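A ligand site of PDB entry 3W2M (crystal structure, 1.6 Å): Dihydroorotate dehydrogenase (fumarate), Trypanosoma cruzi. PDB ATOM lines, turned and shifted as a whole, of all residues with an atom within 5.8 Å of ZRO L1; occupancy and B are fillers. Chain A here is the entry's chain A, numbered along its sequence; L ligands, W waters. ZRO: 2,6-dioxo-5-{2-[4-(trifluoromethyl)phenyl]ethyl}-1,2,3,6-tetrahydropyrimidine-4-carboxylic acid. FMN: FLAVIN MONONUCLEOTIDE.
A nitrogen (NAO) of ZRO L1 lies close to a nitrogen (N1) of FMN L2 (3.4 Å).
OD1 of Asn 128 is in hydrogen-bond range of ND2 of Asn 195. The backbone carbonyl oxygen (O) of Met 70 lies within hydrogen-bond range of the backbone NH (N) of Asn 54 (2.9 Å). O of Ser 69 is in hydrogen-bond range of ND2 of Asn 54, 2.9 Å away. The side-chain amide oxygen of Asn 68 lies within hydrogen-bond range of the backbone NH of Met 70 (3.3 Å). O of Asn 68 lies within hydrogen-bond range of N of Gly 220 (2.9 Å). ND2 of Asn 128 sits at hydrogen-bond distance from OG of Ser 45, 3.4 Å away. The side-chain hydroxyl of Ser 196 is in hydrogen-bond range of the side-chain amide oxygen of Asn 195. The side-chain amide oxygen of Asn 128 is in hydrogen-bond range of the backbone NH of Ser 130 (3.0 Å).
A fluorine (FAG) of ZRO L1 lies close to the side-chain amino group (NZ) of Lys 215 (3.2 Å). Merely in contact with ZRO L1: Asn 54, Ser 69, Ser 130 and Pro 132. Within 4 Å of ZRO L1: Lys 44, Asn 54, Asn 68, Ser 69, Met 70, Gly 71, Leu 72, Asn 128, Ser 130, Pro 132, Asn 195, Ser 196 and Lys 215.
An oxygen (OAB) of ZRO L1 is in hydrogen-bond range of the side-chain amide nitrogen of Asn 68, at 2.9 Å. An oxygen (O2') of FMN L2 is in hydrogen-bond range of the side-chain amino group (NZ) of Lys 165. An oxygen (OAA) of ZRO L1 is in salt-bridge range of the side-chain amino group (NZ) of Lys 44 (3.1 Å). The backbone NH (N) of Met 70 lies within hydrogen-bond range of an oxygen (OAD) of ZRO L1, at 3.1 Å. OD1 of Asn 195 sits at hydrogen-bond distance from NAO of ZRO L1, 2.8 Å away. An oxygen (OAD) of ZRO L1 is in hydrogen-bond range of the backbone NH (N) of Gly 71 (3.0 Å). An oxygen (OAA) of ZRO L1 is in hydrogen-bond range of the backbone NH (N) of Leu 72 (2.8 Å). An oxygen (OAC) of ZRO L1 is in hydrogen-bond range of the side-chain amide nitrogen of Asn 128. The side-chain hydroxyl (OG) of Ser 45 sits at hydrogen-bond distance from a nitrogen (N3) of FMN L2 (2.8 Å). An oxygen (O2) of FMN L2 sits at hydrogen-bond distance from the side-chain amide nitrogen (ND2) of Asn 195. An oxygen (OAB) of ZRO L1 lies within hydrogen-bond range of the side-chain hydroxyl (OG) of Ser 196, at 2.8 Å. The side-chain amino group (NZ) of Lys 44 lies within hydrogen-bond range of an oxygen (O4) of FMN L2 (2.8 Å). The side-chain amide nitrogen of Asn 128 lies within hydrogen-bond range of an oxygen (O2) of FMN L2 (3.3 Å).
Water W2 lies within hydrogen-bond range of an oxygen (OAD) of ZRO L1 and the backbone carbonyl oxygen of Asn 68. Water W1 bridges OG of Ser 69 (2.9 Å) and NZ of Lys 215 (3.1 Å).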
ATOM      1  N   LYS A  44     -13.611   1.394   7.850  1.00  0.00           N
ATOM      2  CA  LYS A  44     -14.779   1.559   7.028  1.00  0.00           C
ATOM      3  C   LYS A  44     -14.539   0.920   5.654  1.00  0.00           C
ATOM      4  O   LYS A  44     -13.523   1.216   5.051  1.00  0.00           O
ATOM      5  CB  LYS A  44     -15.053   3.067   6.895  1.00  0.00           C
ATOM      6  CG  LYS A  44     -16.125   3.396   5.897  1.00  0.00           C
ATOM      7  CD  LYS A  44     -17.566   3.020   6.243  1.00  0.00           C
ATOM      8  CE  LYS A  44     -18.527   3.037   5.025  1.00  0.00           C
ATOM      9  NZ  LYS A  44     -20.027   2.652   5.343  1.00  0.00           N
ATOM     10  N   SER A  45     -15.543   0.217   5.169  1.00  0.00           N
ATOM     11  CA  SER A  45     -15.481  -0.336   3.787  1.00  0.00           C
ATOM     12  C   SER A  45     -15.168   0.832   2.853  1.00  0.00           C
ATOM     13  O   SER A  45     -15.811   1.852   2.888  1.00  0.00           O
ATOM     14  CB  SER A  45     -16.730  -0.974   3.323  1.00  0.00           C
ATOM     15  OG  SER A  45     -16.957  -2.165   4.042  1.00  0.00           O
ATOM     16  N   ASN A  54     -24.674   9.046   0.819  1.00  0.00           N
ATOM     17  CA  ASN A  54     -26.018   9.527   0.573  1.00  0.00           C
ATOM     18  C   ASN A  54     -26.416  10.727   1.425  1.00  0.00           C
ATOM     19  O   ASN A  54     -25.793  11.044   2.383  1.00  0.00           O
ATOM     20  CB  ASN A  54     -26.982   8.418   0.888  1.00  0.00           C
ATOM     21  CG  ASN A  54     -27.036   7.354  -0.134  1.00  0.00           C
ATOM     22  OD1 ASN A  54     -26.643   7.572  -1.332  1.00  0.00           O
ATOM     23  ND2 ASN A  54     -27.404   6.145   0.254  1.00  0.00           N
ATOM     24  N   ASN A  68     -30.020   1.997   8.263  1.00  0.00           N
ATOM     25  CA  ASN A  68     -29.045   2.881   7.635  1.00  0.00           C
ATOM     26  C   ASN A  68     -29.114   2.650   6.130  1.00  0.00           C
ATOM     27  O   ASN A  68     -29.195   1.537   5.620  1.00  0.00           O
ATOM     28  CB  ASN A  68     -27.648   2.734   8.152  1.00  0.00           C
ATOM     29  CG  ASN A  68     -26.884   1.648   7.459  1.00  0.00           C
ATOM     30  OD1 ASN A  68     -26.274   1.865   6.374  1.00  0.00           O
ATOM     31  ND2 ASN A  68     -26.755   0.530   8.091  1.00  0.00           N
ATOM     32  N   SER A  69     -28.865   3.732   5.413  1.00  0.00           N
ATOM     33  CA  SER A  69     -28.561   3.724   3.994  1.00  0.00           C
ATOM     34  C   SER A  69     -27.437   4.724   3.768  1.00  0.00           C
ATOM     35  O   SER A  69     -27.634   5.756   3.136  1.00  0.00           O
ATOM     36  CB  SER A  69     -29.773   3.975   3.111  1.00  0.00           C
ATOM     37  OG  SER A  69     -30.591   2.825   3.087  1.00  0.00           O
ATOM     38  N   MET A  70     -26.278   4.424   4.326  1.00  0.00           N
ATOM     39  CA  MET A  70     -25.186   5.389   4.336  1.00  0.00           C
ATOM     40  C   MET A  70     -24.684   5.712   2.932  1.00  0.00           C
ATOM     41  O   MET A  70     -24.308   6.845   2.628  1.00  0.00           O
ATOM     42  CB  MET A  70     -24.070   4.900   5.164  1.00  0.00           C
ATOM     43  CG  MET A  70     -24.226   4.565   6.587  1.00  0.00           C
ATOM     44  SD  MET A  70     -24.939   5.880   7.570  1.00  0.00           S
ATOM     45  CE  MET A  70     -23.581   6.893   7.833  1.00  0.00           C
ATOM     46  N   GLY A  71     -24.656   4.712   2.029  1.00  0.00           N
ATOM     47  CA  GLY A  71     -24.115   4.912   0.668  1.00  0.00           C
ATOM     48  C   GLY A  71     -22.619   4.872   0.587  1.00  0.00           C
ATOM     49  O   GLY A  71     -22.033   5.560  -0.238  1.00  0.00           O
ATOM     50  N   LEU A  72     -21.953   4.180   1.471  1.00  0.00           N
ATOM     51  CA  LEU A  72     -20.539   4.040   1.468  1.00  0.00           C
ATOM     52  C   LEU A  72     -19.740   5.352   1.492  1.00  0.00           C
ATOM     53  O   LEU A  72     -18.726   5.507   0.790  1.00  0.00           O
ATOM     54  CB  LEU A  72     -20.076   3.197   0.242  1.00  0.00           C
ATOM     55  CG  LEU A  72     -19.138   2.015   0.221  1.00  0.00           C
ATOM     56  CD1 LEU A  72     -18.940   1.216   1.480  1.00  0.00           C
ATOM     57  CD2 LEU A  72     -19.504   1.123  -1.016  1.00  0.00           C
ATOM     58  N   PRO A  73     -20.051   6.255   2.385  1.00  0.00           N
ATOM     59  CA  PRO A  73     -19.192   7.427   2.634  1.00  0.00           C
ATOM     60  C   PRO A  73     -17.856   6.930   3.167  1.00  0.00           C
ATOM     61  O   PRO A  73     -17.775   6.112   4.088  1.00  0.00           O
ATOM     62  CB  PRO A  73     -19.944   8.237   3.662  1.00  0.00           C
ATOM     63  CG  PRO A  73     -20.767   7.289   4.373  1.00  0.00           C
ATOM     64  CD  PRO A  73     -21.031   6.082   3.456  1.00  0.00           C
ATOM     65  N   SER A 100     -14.904  -2.454  -0.335  1.00  0.00           N
ATOM     66  CA  SER A 100     -16.183  -2.661  -0.947  1.00  0.00           C
ATOM     67  C   SER A 100     -16.249  -1.924  -2.279  1.00  0.00           C
ATOM     68  O   SER A 100     -17.035  -1.009  -2.499  1.00  0.00           O
ATOM     69  CB  SER A 100     -17.247  -2.193   0.040  1.00  0.00           C
ATOM     70  OG  SER A 100     -18.503  -2.304  -0.594  1.00  0.00           O
ATOM     71  N   ASN A 128     -16.073  -6.980   1.541  1.00  0.00           N
ATOM     72  CA  ASN A 128     -17.477  -6.850   1.733  1.00  0.00           C
ATOM     73  C   ASN A 128     -18.259  -7.288   0.523  1.00  0.00           C
ATOM     74  O   ASN A 128     -18.221  -6.617  -0.474  1.00  0.00           O
ATOM     75  CB  ASN A 128     -17.779  -5.437   2.108  1.00  0.00           C
ATOM     76  CG  ASN A 128     -19.253  -5.210   2.381  1.00  0.00           C
ATOM     77  OD1 ASN A 128     -20.039  -6.072   2.459  1.00  0.00           O
ATOM     78  ND2 ASN A 128     -19.513  -3.932   2.695  1.00  0.00           N
ATOM     79  N   SER A 130     -21.517  -7.775   0.553  1.00  0.00           N
ATOM     80  CA  SER A 130     -22.906  -7.468   0.756  1.00  0.00           C
ATOM     81  C   SER A 130     -23.000  -6.112   0.321  1.00  0.00           C
ATOM     82  O   SER A 130     -23.148  -5.213   1.048  1.00  0.00           O
ATOM     83  CB  SER A 130     -23.363  -7.644   2.187  1.00  0.00           C
ATOM     84  OG  SER A 130     -24.567  -7.063   2.317  1.00  0.00           O
ATOM     85  N   CYS A 131     -22.872  -5.999  -0.957  1.00  0.00           N
ATOM     86  CA  CYS A 131     -22.622  -4.817  -1.571  1.00  0.00           C
ATOM     87  C   CYS A 131     -23.107  -4.770  -3.078  1.00  0.00           C
ATOM     88  O   CYS A 131     -23.013  -5.674  -3.812  1.00  0.00           O
ATOM     89  CB  CYS A 131     -21.128  -4.853  -1.643  1.00  0.00           C
ATOM     90  SG  CYS A 131     -20.281  -3.534  -2.524  1.00  0.00           S
ATOM     91  N   PRO A 132     -23.470  -3.474  -3.460  1.00  0.00           N
ATOM     92  CA  PRO A 132     -23.812  -3.282  -4.868  1.00  0.00           C
ATOM     93  C   PRO A 132     -22.915  -3.768  -6.006  1.00  0.00           C
ATOM     94  O   PRO A 132     -21.785  -3.580  -6.083  1.00  0.00           O
ATOM     95  CB  PRO A 132     -23.761  -1.726  -4.997  1.00  0.00           C
ATOM     96  CG  PRO A 132     -23.338  -1.137  -3.699  1.00  0.00           C
ATOM     97  CD  PRO A 132     -23.821  -2.136  -2.750  1.00  0.00           C
ATOM     98  N   LYS A 165     -17.160 -10.566   4.328  1.00  0.00           N
ATOM     99  CA  LYS A 165     -18.342 -10.078   5.136  1.00  0.00           C
ATOM    100  C   LYS A 165     -19.594 -10.458   4.291  1.00  0.00           C
ATOM    101  O   LYS A 165     -19.736 -10.084   3.128  1.00  0.00           O
ATOM    102  CB  LYS A 165     -18.300  -8.602   5.306  1.00  0.00           C
ATOM    103  CG  LYS A 165     -19.469  -7.950   6.086  1.00  0.00           C
ATOM    104  CD  LYS A 165     -19.475  -8.219   7.541  1.00  0.00           C
ATOM    105  CE  LYS A 165     -20.476  -7.386   8.248  1.00  0.00           C
ATOM    106  NZ  LYS A 165     -20.042  -5.986   8.361  1.00  0.00           N
ATOM    107  N   ASN A 195     -23.848  -8.950   7.770  1.00  0.00           N
ATOM    108  CA  ASN A 195     -24.085  -7.554   7.502  1.00  0.00           C
ATOM    109  C   ASN A 195     -25.568  -7.290   7.846  1.00  0.00           C
ATOM    110  O   ASN A 195     -26.207  -8.129   8.276  1.00  0.00           O
ATOM    111  CB  ASN A 195     -23.818  -7.301   6.020  1.00  0.00           C
ATOM    112  CG  ASN A 195     -23.361  -5.902   5.737  1.00  0.00           C
ATOM    113  OD1 ASN A 195     -23.943  -4.985   6.146  1.00  0.00           O
ATOM    114  ND2 ASN A 195     -22.291  -5.798   5.010  1.00  0.00           N
ATOM    115  N   SER A 196     -26.012  -6.079   7.592  1.00  0.00           N
ATOM    116  CA  SER A 196     -27.353  -5.718   7.989  1.00  0.00           C
ATOM    117  C   SER A 196     -28.445  -6.524   7.289  1.00  0.00           C
ATOM    118  O   SER A 196     -28.244  -7.037   6.262  1.00  0.00           O
ATOM    119  CB  SER A 196     -27.561  -4.185   7.835  1.00  0.00           C
ATOM    120  OG  SER A 196     -27.075  -3.692   6.667  1.00  0.00           O
ATOM    121  N   LYS A 215     -33.468   6.202  -0.642  1.00  0.00           N
ATOM    122  CA  LYS A 215     -34.218   4.948  -0.983  1.00  0.00           C
ATOM    123  C   LYS A 215     -35.608   4.957  -0.385  1.00  0.00           C
ATOM    124  O   LYS A 215     -36.138   3.899  -0.027  1.00  0.00           O
ATOM    125  CB  LYS A 215     -33.424   3.713  -0.499  1.00  0.00           C
ATOM    126  CG  LYS A 215     -32.099   3.528  -1.203  1.00  0.00           C
ATOM    127  CD  LYS A 215     -31.242   2.394  -0.573  1.00  0.00           C
ATOM    128  CE  LYS A 215     -32.049   1.133  -0.477  1.00  0.00           C
ATOM    129  NZ  LYS A 215     -31.111  -0.040  -0.295  1.00  0.00           N
ATOM    130  N   GLY A 220     -30.737  -0.869   5.629  1.00  0.00           N
ATOM    131  CA  GLY A 220     -30.349  -2.073   6.326  1.00  0.00           C
ATOM    132  C   GLY A 220     -30.550  -1.997   7.834  1.00  0.00           C
ATOM    133  O   GLY A 220     -30.266  -0.986   8.438  1.00  0.00           O
HETATM  134  OAA ZRO L   1     -22.425   2.239   3.464  1.00  0.00           O
HETATM  135  CAP ZRO L   1     -23.476   1.630   3.639  1.00  0.00           C
HETATM  136  OAD ZRO L   1     -24.595   1.989   3.347  1.00  0.00           O
HETATM  137  CAS ZRO L   1     -23.432   0.187   4.164  1.00  0.00           C
HETATM  138  NAN ZRO L   1     -24.291  -0.072   5.212  1.00  0.00           N
HETATM  139  CAU ZRO L   1     -24.415  -1.317   5.774  1.00  0.00           C
HETATM  140  OAB ZRO L   1     -25.293  -1.576   6.658  1.00  0.00           O
HETATM  141  NAO ZRO L   1     -23.658  -2.333   5.292  1.00  0.00           N
HETATM  142  CAV ZRO L   1     -22.772  -2.131   4.204  1.00  0.00           C
HETATM  143  OAC ZRO L   1     -22.048  -3.075   3.840  1.00  0.00           O
HETATM  144  CAT ZRO L   1     -22.715  -0.831   3.632  1.00  0.00           C
HETATM  145  CAM ZRO L   1     -21.800  -0.637   2.585  1.00  0.00           C
HETATM  146  CAL ZRO L   1     -22.299  -1.345   1.244  1.00  0.00           C
HETATM  147  CAQ ZRO L   1     -23.407  -0.669   0.735  1.00  0.00           C
HETATM  148  CAH ZRO L   1     -23.316   0.424  -0.099  1.00  0.00           C
HETATM  149  CAJ ZRO L   1     -24.443   1.141  -0.572  1.00  0.00           C
HETATM  150  CAR ZRO L   1     -25.737   0.875  -0.059  1.00  0.00           C
HETATM  151  CAW ZRO L   1     -26.939   1.683  -0.405  1.00  0.00           C
HETATM  152  FAF ZRO L   1     -26.750   2.558  -1.389  1.00  0.00           F
HETATM  153  FAG ZRO L   1     -28.030   0.880  -0.639  1.00  0.00           F
HETATM  154  FAE ZRO L   1     -27.155   2.674   0.741  1.00  0.00           F
HETATM  155  CAK ZRO L   1     -25.845  -0.214   0.837  1.00  0.00           C
HETATM  156  CAI ZRO L   1     -24.712  -0.996   1.183  1.00  0.00           C
HETATM  157  N1  FMN L   2     -20.853  -3.250   7.042  1.00  0.00           N
HETATM  158  C2  FMN L   2     -19.800  -3.339   6.180  1.00  0.00           C
HETATM  159  O2  FMN L   2     -19.302  -4.472   5.969  1.00  0.00           O
HETATM  160  N3  FMN L   2     -19.200  -2.235   5.697  1.00  0.00           N
HETATM  161  C4  FMN L   2     -19.633  -0.976   5.958  1.00  0.00           C
HETATM  162  O4  FMN L   2     -19.033   0.067   5.531  1.00  0.00           O
HETATM  163  C4A FMN L   2     -20.752  -0.816   6.825  1.00  0.00           C
HETATM  164  N5  FMN L   2     -21.216   0.397   7.151  1.00  0.00           N
HETATM  165  C5A FMN L   2     -22.208   0.497   8.117  1.00  0.00           C
HETATM  166  C6  FMN L   2     -22.543   1.746   8.636  1.00  0.00           C
HETATM  167  C7  FMN L   2     -23.481   1.898   9.656  1.00  0.00           C
HETATM  168  C7M FMN L   2     -23.873   3.275  10.127  1.00  0.00           C
HETATM  169  C8  FMN L   2     -24.094   0.730  10.236  1.00  0.00           C
HETATM  170  C8M FMN L   2     -25.090   0.812  11.317  1.00  0.00           C
HETATM  171  C9  FMN L   2     -23.679  -0.520   9.775  1.00  0.00           C
HETATM  172  C9A FMN L   2     -22.781  -0.686   8.732  1.00  0.00           C
HETATM  173  N10 FMN L   2     -22.373  -1.939   8.216  1.00  0.00           N
HETATM  174  C10 FMN L   2     -21.309  -2.051   7.365  1.00  0.00           C
HETATM  175  C1' FMN L   2     -22.930  -3.142   8.787  1.00  0.00           C
HETATM  176  C2' FMN L   2     -22.361  -3.522  10.153  1.00  0.00           C
HETATM  177  O2' FMN L   2     -20.979  -3.813   9.954  1.00  0.00           O
HETATM  178  C3' FMN L   2     -23.055  -4.701  10.779  1.00  0.00           C
HETATM  179  O3' FMN L   2     -22.839  -5.839   9.873  1.00  0.00           O
HETATM  180  C4' FMN L   2     -24.545  -4.524  10.982  1.00  0.00           C
HETATM  181  O4' FMN L   2     -24.757  -3.205  11.516  1.00  0.00           O
HETATM  182  C5' FMN L   2     -25.068  -5.504  12.015  1.00  0.00           C
HETATM  183  O5' FMN L   2     -24.468  -5.508  13.266  1.00  0.00           O
HETATM  184  P   FMN L   2     -25.202  -4.772  14.541  1.00  0.00           P
HETATM  185  O1P FMN L   2     -24.220  -4.835  15.672  1.00  0.00           O
HETATM  186  O2P FMN L   2     -26.491  -5.490  14.761  1.00  0.00           O
HETATM  187  O3P FMN L   2     -25.517  -3.323  14.066  1.00  0.00           O
HETATM  188  O   HOH W   1     -29.517   0.227   2.350  1.00  0.00           O
HETATM  189  O   HOH W   2     -27.062   0.393   3.727  1.00  0.00           O
HETATM  190  O   HOH W   3     -28.275   4.494  -2.317  1.00  0.00           O
